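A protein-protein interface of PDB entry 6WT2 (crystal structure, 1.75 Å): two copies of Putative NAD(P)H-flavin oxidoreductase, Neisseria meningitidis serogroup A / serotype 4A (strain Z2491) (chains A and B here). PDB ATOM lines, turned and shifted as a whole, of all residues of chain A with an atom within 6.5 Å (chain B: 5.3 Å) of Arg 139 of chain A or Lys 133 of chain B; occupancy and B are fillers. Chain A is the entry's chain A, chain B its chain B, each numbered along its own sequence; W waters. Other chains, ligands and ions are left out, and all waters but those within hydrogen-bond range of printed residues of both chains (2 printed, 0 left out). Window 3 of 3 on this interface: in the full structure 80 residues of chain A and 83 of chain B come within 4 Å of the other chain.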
ATOM      1  N   ILE A 134      42.343 -10.503  15.344  1.00  0.00           N
ATOM      2  CA  ILE A 134      40.887 -10.536  15.333  1.00  0.00           C
ATOM      3  C   ILE A 134      40.281  -9.322  14.632  1.00  0.00           C
ATOM      4  O   ILE A 134      39.069  -9.132  14.684  1.00  0.00           O
ATOM      5  CB  ILE A 134      40.321 -10.675  16.762  1.00  0.00           C
ATOM      6  CG1 ILE A 134      40.812  -9.521  17.656  1.00  0.00           C
ATOM      7  CG2 ILE A 134      40.655 -12.041  17.345  1.00  0.00           C
ATOM      8  CD1 ILE A 134      40.212  -9.528  19.058  1.00  0.00           C
ATOM      9  N   ASP A 137      38.096  -9.957  10.851  1.00  0.00           N
ATOM     10  CA  ASP A 137      36.819 -10.658  10.810  1.00  0.00           C
ATOM     11  C   ASP A 137      35.978 -10.215  11.997  1.00  0.00           C
ATOM     12  O   ASP A 137      36.413 -10.332  13.147  1.00  0.00           O
ATOM     13  CB  ASP A 137      37.033 -12.174  10.831  1.00  0.00           C
ATOM     14  CG  ASP A 137      35.731 -12.951  10.850  1.00  0.00           C
ATOM     15  OD1 ASP A 137      34.689 -12.409  10.420  1.00  0.00           O
ATOM     16  OD2 ASP A 137      35.750 -14.112  11.308  1.00  0.00           O
ATOM     17  N   SER A 138      34.773  -9.712  11.720  1.00  0.00           N
ATOM     18  CA  SER A 138      33.871  -9.317  12.797  1.00  0.00           C
ATOM     19  C   SER A 138      33.471 -10.507  13.662  1.00  0.00           C
ATOM     20  O   SER A 138      33.199 -10.339  14.855  1.00  0.00           O
ATOM     21  CB  SER A 138      32.626  -8.643  12.220  1.00  0.00           C
ATOM     22  OG  SER A 138      31.871  -9.570  11.461  1.00  0.00           O
ATOM     23  N   ARG A 139      33.432 -11.716  13.089  1.00  0.00           N
ATOM     24  CA  ARG A 139      33.080 -12.886  13.891  1.00  0.00           C
ATOM     25  C   ARG A 139      34.197 -13.250  14.862  1.00  0.00           C
ATOM     26  O   ARG A 139      33.927 -13.654  16.000  1.00  0.00           O
ATOM     27  CB  ARG A 139      32.743 -14.081  12.993  1.00  0.00           C
ATOM     28  CG  ARG A 139      31.837 -15.107  13.676  1.00  0.00           C
ATOM     29  CD  ARG A 139      32.367 -16.544  13.573  1.00  0.00           C
ATOM     30  NE  ARG A 139      31.383 -17.467  13.001  1.00  0.00           N
ATOM     31  CZ  ARG A 139      30.566 -18.241  13.711  1.00  0.00           C
ATOM     32  NH1 ARG A 139      30.599 -18.215  15.037  1.00  0.00           N
ATOM     33  NH2 ARG A 139      29.709 -19.038  13.093  1.00  0.00           N
ATOM     34  N   ALA A 140      35.458 -13.118  14.435  1.00  0.00           N
ATOM     35  CA  ALA A 140      36.573 -13.380  15.344  1.00  0.00           C
ATOM     36  C   ALA A 140      36.598 -12.368  16.480  1.00  0.00           C
ATOM     37  O   ALA A 140      36.867 -12.721  17.636  1.00  0.00           O
ATOM     38  CB  ALA A 140      37.896 -13.361  14.581  1.00  0.00           C
ATOM     39  N   LEU A 141      36.303 -11.106  16.170  1.00  0.00           N
ATOM     40  CA  LEU A 141      36.185 -10.088  17.204  1.00  0.00           C
ATOM     41  C   LEU A 141      35.063 -10.418  18.184  1.00  0.00           C
ATOM     42  O   LEU A 141      35.239 -10.290  19.401  1.00  0.00           O
ATOM     43  CB  LEU A 141      35.965  -8.731  16.536  1.00  0.00           C
ATOM     44  CG  LEU A 141      36.201  -7.398  17.232  1.00  0.00           C
ATOM     45  CD1 LEU A 141      37.440  -7.339  18.107  1.00  0.00           C
ATOM     46  CD2 LEU A 141      36.311  -6.354  16.134  1.00  0.00           C
ATOM     47  N   PHE A 142      33.898 -10.839  17.677  1.00  0.00           N
ATOM     48  CA  PHE A 142      32.804 -11.222  18.568  1.00  0.00           C
ATOM     49  C   PHE A 142      33.180 -12.448  19.398  1.00  0.00           C
ATOM     50  O   PHE A 142      32.893 -12.510  20.601  1.00  0.00           O
ATOM     51  CB  PHE A 142      31.532 -11.479  17.746  1.00  0.00           C
ATOM     52  CG  PHE A 142      30.376 -12.037  18.551  1.00  0.00           C
ATOM     53  CD1 PHE A 142      29.754 -11.273  19.530  1.00  0.00           C
ATOM     54  CD2 PHE A 142      29.902 -13.319  18.308  1.00  0.00           C
ATOM     55  CE1 PHE A 142      28.689 -11.781  20.261  1.00  0.00           C
ATOM     56  CE2 PHE A 142      28.833 -13.834  19.033  1.00  0.00           C
ATOM     57  CZ  PHE A 142      28.233 -13.073  20.012  1.00  0.00           C
ATOM     58  N   ASP A 143      33.836 -13.430  18.772  1.00  0.00           N
ATOM     59  CA  ASP A 143      34.240 -14.640  19.486  1.00  0.00           C
ATOM     60  C   ASP A 143      35.249 -14.337  20.590  1.00  0.00           C
ATOM     61  O   ASP A 143      35.234 -14.997  21.638  1.00  0.00           O
ATOM     62  CB  ASP A 143      34.793 -15.663  18.491  1.00  0.00           C
ATOM     63  CG  ASP A 143      33.691 -16.564  17.895  1.00  0.00           C
ATOM     64  OD1 ASP A 143      32.533 -16.514  18.385  1.00  0.00           O
ATOM     65  OD2 ASP A 143      33.979 -17.331  16.941  1.00  0.00           O
ATOM     66  N   TRP A 144      36.125 -13.348  20.374  1.00  0.00           N
ATOM     67  CA  TRP A 144      37.009 -12.868  21.434  1.00  0.00           C
ATOM     68  C   TRP A 144      36.221 -12.446  22.670  1.00  0.00           C
ATOM     69  O   TRP A 144      36.531 -12.860  23.794  1.00  0.00           O
ATOM     70  CB  TRP A 144      37.860 -11.709  20.910  1.00  0.00           C
ATOM     71  CG  TRP A 144      38.794 -11.112  21.931  1.00  0.00           C
ATOM     72  CD1 TRP A 144      39.752 -11.766  22.657  1.00  0.00           C
ATOM     73  CD2 TRP A 144      38.860  -9.736  22.327  1.00  0.00           C
ATOM     74  NE1 TRP A 144      40.407 -10.875  23.491  1.00  0.00           N
ATOM     75  CE2 TRP A 144      39.873  -9.626  23.303  1.00  0.00           C
ATOM     76  CE3 TRP A 144      38.149  -8.586  21.957  1.00  0.00           C
ATOM     77  CZ2 TRP A 144      40.199  -8.412  23.906  1.00  0.00           C
ATOM     78  CZ3 TRP A 144      38.470  -7.385  22.562  1.00  0.00           C
ATOM     79  CH2 TRP A 144      39.495  -7.304  23.520  1.00  0.00           C
ATOM     80  N   ASN A 174      18.932 -22.755  19.484  1.00  0.00           N
ATOM     81  CA  ASN A 174      19.208 -22.092  18.219  1.00  0.00           C
ATOM     82  C   ASN A 174      19.629 -20.655  18.494  1.00  0.00           C
ATOM     83  O   ASN A 174      18.853 -19.859  19.037  1.00  0.00           O
ATOM     84  CB  ASN A 174      17.992 -22.143  17.299  1.00  0.00           C
ATOM     85  CG  ASN A 174      18.300 -21.609  15.914  1.00  0.00           C
ATOM     86  OD1 ASN A 174      18.297 -20.400  15.690  1.00  0.00           O
ATOM     87  ND2 ASN A 174      18.578 -22.507  14.980  1.00  0.00           N
ATOM     88  N   TYR A 175      20.866 -20.323  18.137  1.00  0.00           N
ATOM     89  CA  TYR A 175      21.403 -19.022  18.527  1.00  0.00           C
ATOM     90  C   TYR A 175      20.729 -17.882  17.771  1.00  0.00           C
ATOM     91  O   TYR A 175      20.481 -16.813  18.344  1.00  0.00           O
ATOM     92  CB  TYR A 175      22.911 -19.000  18.304  1.00  0.00           C
ATOM     93  CG  TYR A 175      23.689 -19.441  19.515  1.00  0.00           C
ATOM     94  CD1 TYR A 175      24.496 -18.545  20.204  1.00  0.00           C
ATOM     95  CD2 TYR A 175      23.604 -20.757  19.983  1.00  0.00           C
ATOM     96  CE1 TYR A 175      25.223 -18.944  21.322  1.00  0.00           C
ATOM     97  CE2 TYR A 175      24.326 -21.165  21.106  1.00  0.00           C
ATOM     98  CZ  TYR A 175      25.139 -20.259  21.762  1.00  0.00           C
ATOM     99  OH  TYR A 175      25.844 -20.651  22.880  1.00  0.00           O
ATOM    100  N   ALA A 176      20.431 -18.086  16.486  1.00  0.00           N
ATOM    101  CA  ALA A 176      19.749 -17.047  15.714  1.00  0.00           C
ATOM    102  C   ALA A 176      18.334 -16.802  16.233  1.00  0.00           C
ATOM    103  O   ALA A 176      17.882 -15.651  16.305  1.00  0.00           O
ATOM    104  CB  ALA A 176      19.723 -17.435  14.235  1.00  0.00           C
ATOM    105  N   PHE B 127      23.209 -29.917  16.509  1.00  0.00           N
ATOM    106  CA  PHE B 127      23.687 -28.800  17.318  1.00  0.00           C
ATOM    107  C   PHE B 127      24.777 -28.026  16.589  1.00  0.00           C
ATOM    108  O   PHE B 127      24.699 -26.799  16.450  1.00  0.00           O
ATOM    109  CB  PHE B 127      24.198 -29.319  18.667  1.00  0.00           C
ATOM    110  CG  PHE B 127      24.955 -28.297  19.458  1.00  0.00           C
ATOM    111  CD1 PHE B 127      24.314 -27.158  19.943  1.00  0.00           C
ATOM    112  CD2 PHE B 127      26.301 -28.473  19.722  1.00  0.00           C
ATOM    113  CE1 PHE B 127      25.006 -26.207  20.678  1.00  0.00           C
ATOM    114  CE2 PHE B 127      27.011 -27.531  20.457  1.00  0.00           C
ATOM    115  CZ  PHE B 127      26.364 -26.393  20.935  1.00  0.00           C
ATOM    116  N   GLN B 128      25.800 -28.729  16.098  1.00  0.00           N
ATOM    117  CA  GLN B 128      26.933 -28.029  15.495  1.00  0.00           C
ATOM    118  C   GLN B 128      26.558 -27.384  14.166  1.00  0.00           C
ATOM    119  O   GLN B 128      27.051 -26.302  13.835  1.00  0.00           O
ATOM    120  CB  GLN B 128      28.105 -28.994  15.309  1.00  0.00           C
ATOM    121  CG  GLN B 128      28.726 -29.423  16.617  1.00  0.00           C
ATOM    122  CD  GLN B 128      30.008 -30.190  16.393  1.00  0.00           C
ATOM    123  OE1 GLN B 128      30.122 -30.950  15.430  1.00  0.00           O
ATOM    124  NE2 GLN B 128      30.988 -29.979  17.268  1.00  0.00           N
ATOM    125  N   ALA B 129      25.697 -28.032  13.389  1.00  0.00           N
ATOM    126  CA  ALA B 129      25.370 -27.525  12.063  1.00  0.00           C
ATOM    127  C   ALA B 129      24.239 -26.502  12.088  1.00  0.00           C
ATOM    128  O   ALA B 129      24.272 -25.525  11.331  1.00  0.00           O
ATOM    129  CB  ALA B 129      24.988 -28.684  11.136  1.00  0.00           C
ATOM    130  N   ASP B 130      23.228 -26.708  12.926  1.00  0.00           N
ATOM    131  CA  ASP B 130      22.002 -25.934  12.824  1.00  0.00           C
ATOM    132  C   ASP B 130      21.820 -24.911  13.934  1.00  0.00           C
ATOM    133  O   ASP B 130      21.230 -23.856  13.690  1.00  0.00           O
ATOM    134  CB  ASP B 130      20.781 -26.867  12.810  1.00  0.00           C
ATOM    135  CG  ASP B 130      20.867 -27.948  11.730  1.00  0.00           C
ATOM    136  OD1 ASP B 130      21.553 -27.729  10.706  1.00  0.00           O
ATOM    137  OD2 ASP B 130      20.234 -29.017  11.904  1.00  0.00           O
ATOM    138  N   ASP B 131      22.296 -25.199  15.143  1.00  0.00           N
ATOM    139  CA  ASP B 131      22.006 -24.367  16.302  1.00  0.00           C
ATOM    140  C   ASP B 131      23.109 -23.352  16.565  1.00  0.00           C
ATOM    141  O   ASP B 131      22.842 -22.153  16.585  1.00  0.00           O
ATOM    142  CB  ASP B 131      21.771 -25.237  17.543  1.00  0.00           C
ATOM    143  CG  ASP B 131      20.460 -25.991  17.474  1.00  0.00           C
ATOM    144  OD1 ASP B 131      19.537 -25.502  16.778  1.00  0.00           O
ATOM    145  OD2 ASP B 131      20.349 -27.060  18.109  1.00  0.00           O
ATOM    146  N   ILE B 132      24.343 -23.810  16.793  1.00  0.00           N
ATOM    147  CA  ILE B 132      25.449 -22.879  17.000  1.00  0.00           C
ATOM    148  C   ILE B 132      26.237 -22.617  15.722  1.00  0.00           C
ATOM    149  O   ILE B 132      27.015 -21.650  15.677  1.00  0.00           O
ATOM    150  CB  ILE B 132      26.360 -23.385  18.139  1.00  0.00           C
ATOM    151  CG1 ILE B 132      27.194 -22.233  18.708  1.00  0.00           C
ATOM    152  CG2 ILE B 132      27.250 -24.540  17.669  1.00  0.00           C
ATOM    153  CD1 ILE B 132      27.878 -22.588  20.012  1.00  0.00           C
ATOM    154  N   LYS B 133      26.046 -23.432  14.678  1.00  0.00           N
ATOM    155  CA  LYS B 133      26.508 -23.134  13.317  1.00  0.00           C
ATOM    156  C   LYS B 133      28.027 -22.955  13.268  1.00  0.00           C
ATOM    157  O   LYS B 133      28.556 -21.901  12.903  1.00  0.00           O
ATOM    158  CB  LYS B 133      25.784 -21.903  12.754  1.00  0.00           C
ATOM    159  CG  LYS B 133      24.323 -22.161  12.444  1.00  0.00           C
ATOM    160  CD  LYS B 133      23.856 -21.298  11.288  1.00  0.00           C
ATOM    161  CE  LYS B 133      22.784 -22.002  10.493  1.00  0.00           C
ATOM    162  NZ  LYS B 133      23.248 -23.345  10.026  1.00  0.00           N
ATOM    163  N   ILE B 134      28.727 -24.014  13.664  1.00  0.00           N
ATOM    164  CA  ILE B 134      30.184 -24.025  13.668  1.00  0.00           C
ATOM    165  C   ILE B 134      30.761 -25.130  12.800  1.00  0.00           C
ATOM    166  O   ILE B 134      31.971 -25.123  12.545  1.00  0.00           O
ATOM    167  CB  ILE B 134      30.743 -24.147  15.103  1.00  0.00           C
ATOM    168  CG1 ILE B 134      30.366 -25.512  15.692  1.00  0.00           C
ATOM    169  CG2 ILE B 134      30.250 -22.999  15.969  1.00  0.00           C
ATOM    170  CD1 ILE B 134      30.956 -25.797  17.072  1.00  0.00           C
ATOM    171  N   LEU B 135      29.945 -26.075  12.331  1.00  0.00           N
ATOM    172  CA  LEU B 135      30.475 -27.220  11.594  1.00  0.00           C
ATOM    173  C   LEU B 135      31.105 -26.791  10.277  1.00  0.00           C
ATOM    174  O   LEU B 135      32.046 -27.433   9.797  1.00  0.00           O
ATOM    175  CB  LEU B 135      29.360 -28.243  11.351  1.00  0.00           C
ATOM    176  CG  LEU B 135      29.783 -29.669  10.999  1.00  0.00           C
ATOM    177  CD1 LEU B 135      30.567 -30.305  12.150  1.00  0.00           C
ATOM    178  CD2 LEU B 135      28.564 -30.510  10.635  1.00  0.00           C
ATOM    179  N   ASP B 136      30.615 -25.696   9.696  1.00  0.00           N
ATOM    180  CA  ASP B 136      31.129 -25.211   8.421  1.00  0.00           C
ATOM    181  C   ASP B 136      32.568 -24.718   8.550  1.00  0.00           C
ATOM    182  O   ASP B 136      33.435 -25.080   7.747  1.00  0.00           O
ATOM    183  CB  ASP B 136      30.227 -24.083   7.907  1.00  0.00           C
ATOM    184  CG  ASP B 136      29.884 -24.223   6.434  1.00  0.00           C
ATOM    185  OD1 ASP B 136      28.719 -23.951   6.071  1.00  0.00           O
ATOM    186  OD2 ASP B 136      30.769 -24.613   5.642  1.00  0.00           O
ATOM    187  N   ASP B 137      32.838 -23.895   9.561  1.00  0.00           N
ATOM    188  CA  ASP B 137      34.042 -23.076   9.632  1.00  0.00           C
ATOM    189  C   ASP B 137      35.012 -23.671  10.643  1.00  0.00           C
ATOM    190  O   ASP B 137      34.675 -23.810  11.825  1.00  0.00           O
ATOM    191  CB  ASP B 137      33.682 -21.638  10.010  1.00  0.00           C
ATOM    192  CG  ASP B 137      34.820 -20.661   9.772  1.00  0.00           C
ATOM    193  OD1 ASP B 137      36.005 -21.054   9.878  1.00  0.00           O
ATOM    194  OD2 ASP B 137      34.526 -19.484   9.472  1.00  0.00           O
ATOM    195  N   ALA B 140      35.692 -21.264  13.523  1.00  0.00           N
ATOM    196  CA  ALA B 140      34.583 -21.217  14.469  1.00  0.00           C
ATOM    197  C   ALA B 140      34.526 -22.485  15.314  1.00  0.00           C
ATOM    198  O   ALA B 140      34.197 -22.432  16.506  1.00  0.00           O
ATOM    199  CB  ALA B 140      33.261 -21.014  13.728  1.00  0.00           C
ATOM    200  N   ARG B 147      36.418 -21.402  23.824  1.00  0.00           N
ATOM    201  CA  ARG B 147      35.451 -20.943  24.821  1.00  0.00           C
ATOM    202  C   ARG B 147      35.439 -21.845  26.054  1.00  0.00           C
ATOM    203  O   ARG B 147      35.440 -21.358  27.193  1.00  0.00           O
ATOM    204  CB  ARG B 147      34.044 -20.881  24.213  1.00  0.00           C
ATOM    205  CG  ARG B 147      33.830 -19.774  23.197  1.00  0.00           C
ATOM    206  CD  ARG B 147      32.419 -19.869  22.661  1.00  0.00           C
ATOM    207  NE  ARG B 147      32.201 -19.002  21.516  1.00  0.00           N
ATOM    208  CZ  ARG B 147      31.017 -18.475  21.206  1.00  0.00           C
ATOM    209  NH1 ARG B 147      29.959 -18.729  21.971  1.00  0.00           N
ATOM    210  NH2 ARG B 147      30.889 -17.691  20.143  1.00  0.00           N
HETATM  211  O   HOH W   1      19.807 -20.820  12.817  1.00  0.00           O
HETATM  212  O   HOH W   2      21.750 -20.203  14.746  1.00  0.00           O
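OD1 of Asp 143 of chain A lies within salt-bridge range of NH2 of Arg 147 of chain B, at 2.7 Å.
ND2 of Asn 174 of chain A is in hydrogen-bond range of O of Asp 130 of chain B, 3.2 Å away.
O of Asp 131 of chain B is in hydrogen-bond range of N of Tyr 175 of chain A (3.1 Å).
The guanidinium group of Arg 139 of chain A lies within hydrogen-bond range of the backbone carbonyl oxygen of Lys 133 of chain B.
The guanidinium group (NH1) of Arg 139 of chain A is in salt-bridge range of the side-chain carboxylate (OD2) of Asp 143 of chain A, 3.98 Å away.
OD1 of Asp 137 of chain A sits at hydrogen-bond distance from N of Arg 139 of chain A (3.0 Å).
The backbone NH (N) of Ile 132 of chain B is in hydrogen-bond range of the backbone carbonyl oxygen (O) of Phe 127 of chain B (3.0 Å).
O of Gln 128 of chain B is in hydrogen-bond range of N of Lys 133 of chain B, at 3.2 Å.
N of Ala 176 of chain A sits at hydrogen-bond distance from OD1 of Asn 174 of chain A.
The backbone carbonyl oxygen (O) of Ala 129 of chain B sits at hydrogen-bond distance from the side-chain amino group (NZ) of Lys 133 of chain B (2.7 Å).
Ala 140 of chain B touches Arg 139 of chain A (CB to CZ, 3.9 Å).
Asn 174 of chain A touches Asp 131 of chain B.
Tyr 175 of chain A touches Ile 132 of chain B.
Of the printed residues of chain B, Arg 139 of chain A touches Lys 133 and Ala 140.
Of the printed residues of chain A, Lys 133 of chain B touches Arg 139.
Of the printed residues of chain A, Asp 131 of chain B touches Asn 174 and Tyr 175.
Of the printed residues of chain A, Asp 130 of chain B touches Asn 174.
Gln 128 of chain B touches none of the printed residues of chain A.
The nearest printed residue of chain A that does not touch Ile 132 of chain B is Arg 139 of chain A (4.6 Å).
Printed residues of chain B that touch a printed residue of chain A: Asp 130, Asp 131, Ile 132, Lys 133, Ala 140 and Arg 147.
Hydrophobic or aromatic side chains of chain B within 4 Å of the printed part of chain A: Ile 132 and Ala 140.
Along chain B the printed residues that touch a printed residue of chain A span positions 130 to 147.
Hydrophobic or aromatic side chains of chain A that line the printed part of chain B: Tyr 175.
Among the printed residues, Asp or Glu carboxylates within 4 Å of a Lys or Arg side-chain nitrogen of the other chain: Asp 143 of chain A with Arg 147 of chain B (2.7 Å).
3 positions are printed for both chains.
Water W2 lies within hydrogen-bond range of the backbone carbonyl oxygen of Asp 131 of chain B (2.9 Å) and the backbone NH of Ala 176 of chain A (3.0 Å).
Water W1 lies within hydrogen-bond range of ND2 of Asn 174 of chain A (3.0 Å) and O of Asp 130 of chain B (3.5 Å).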
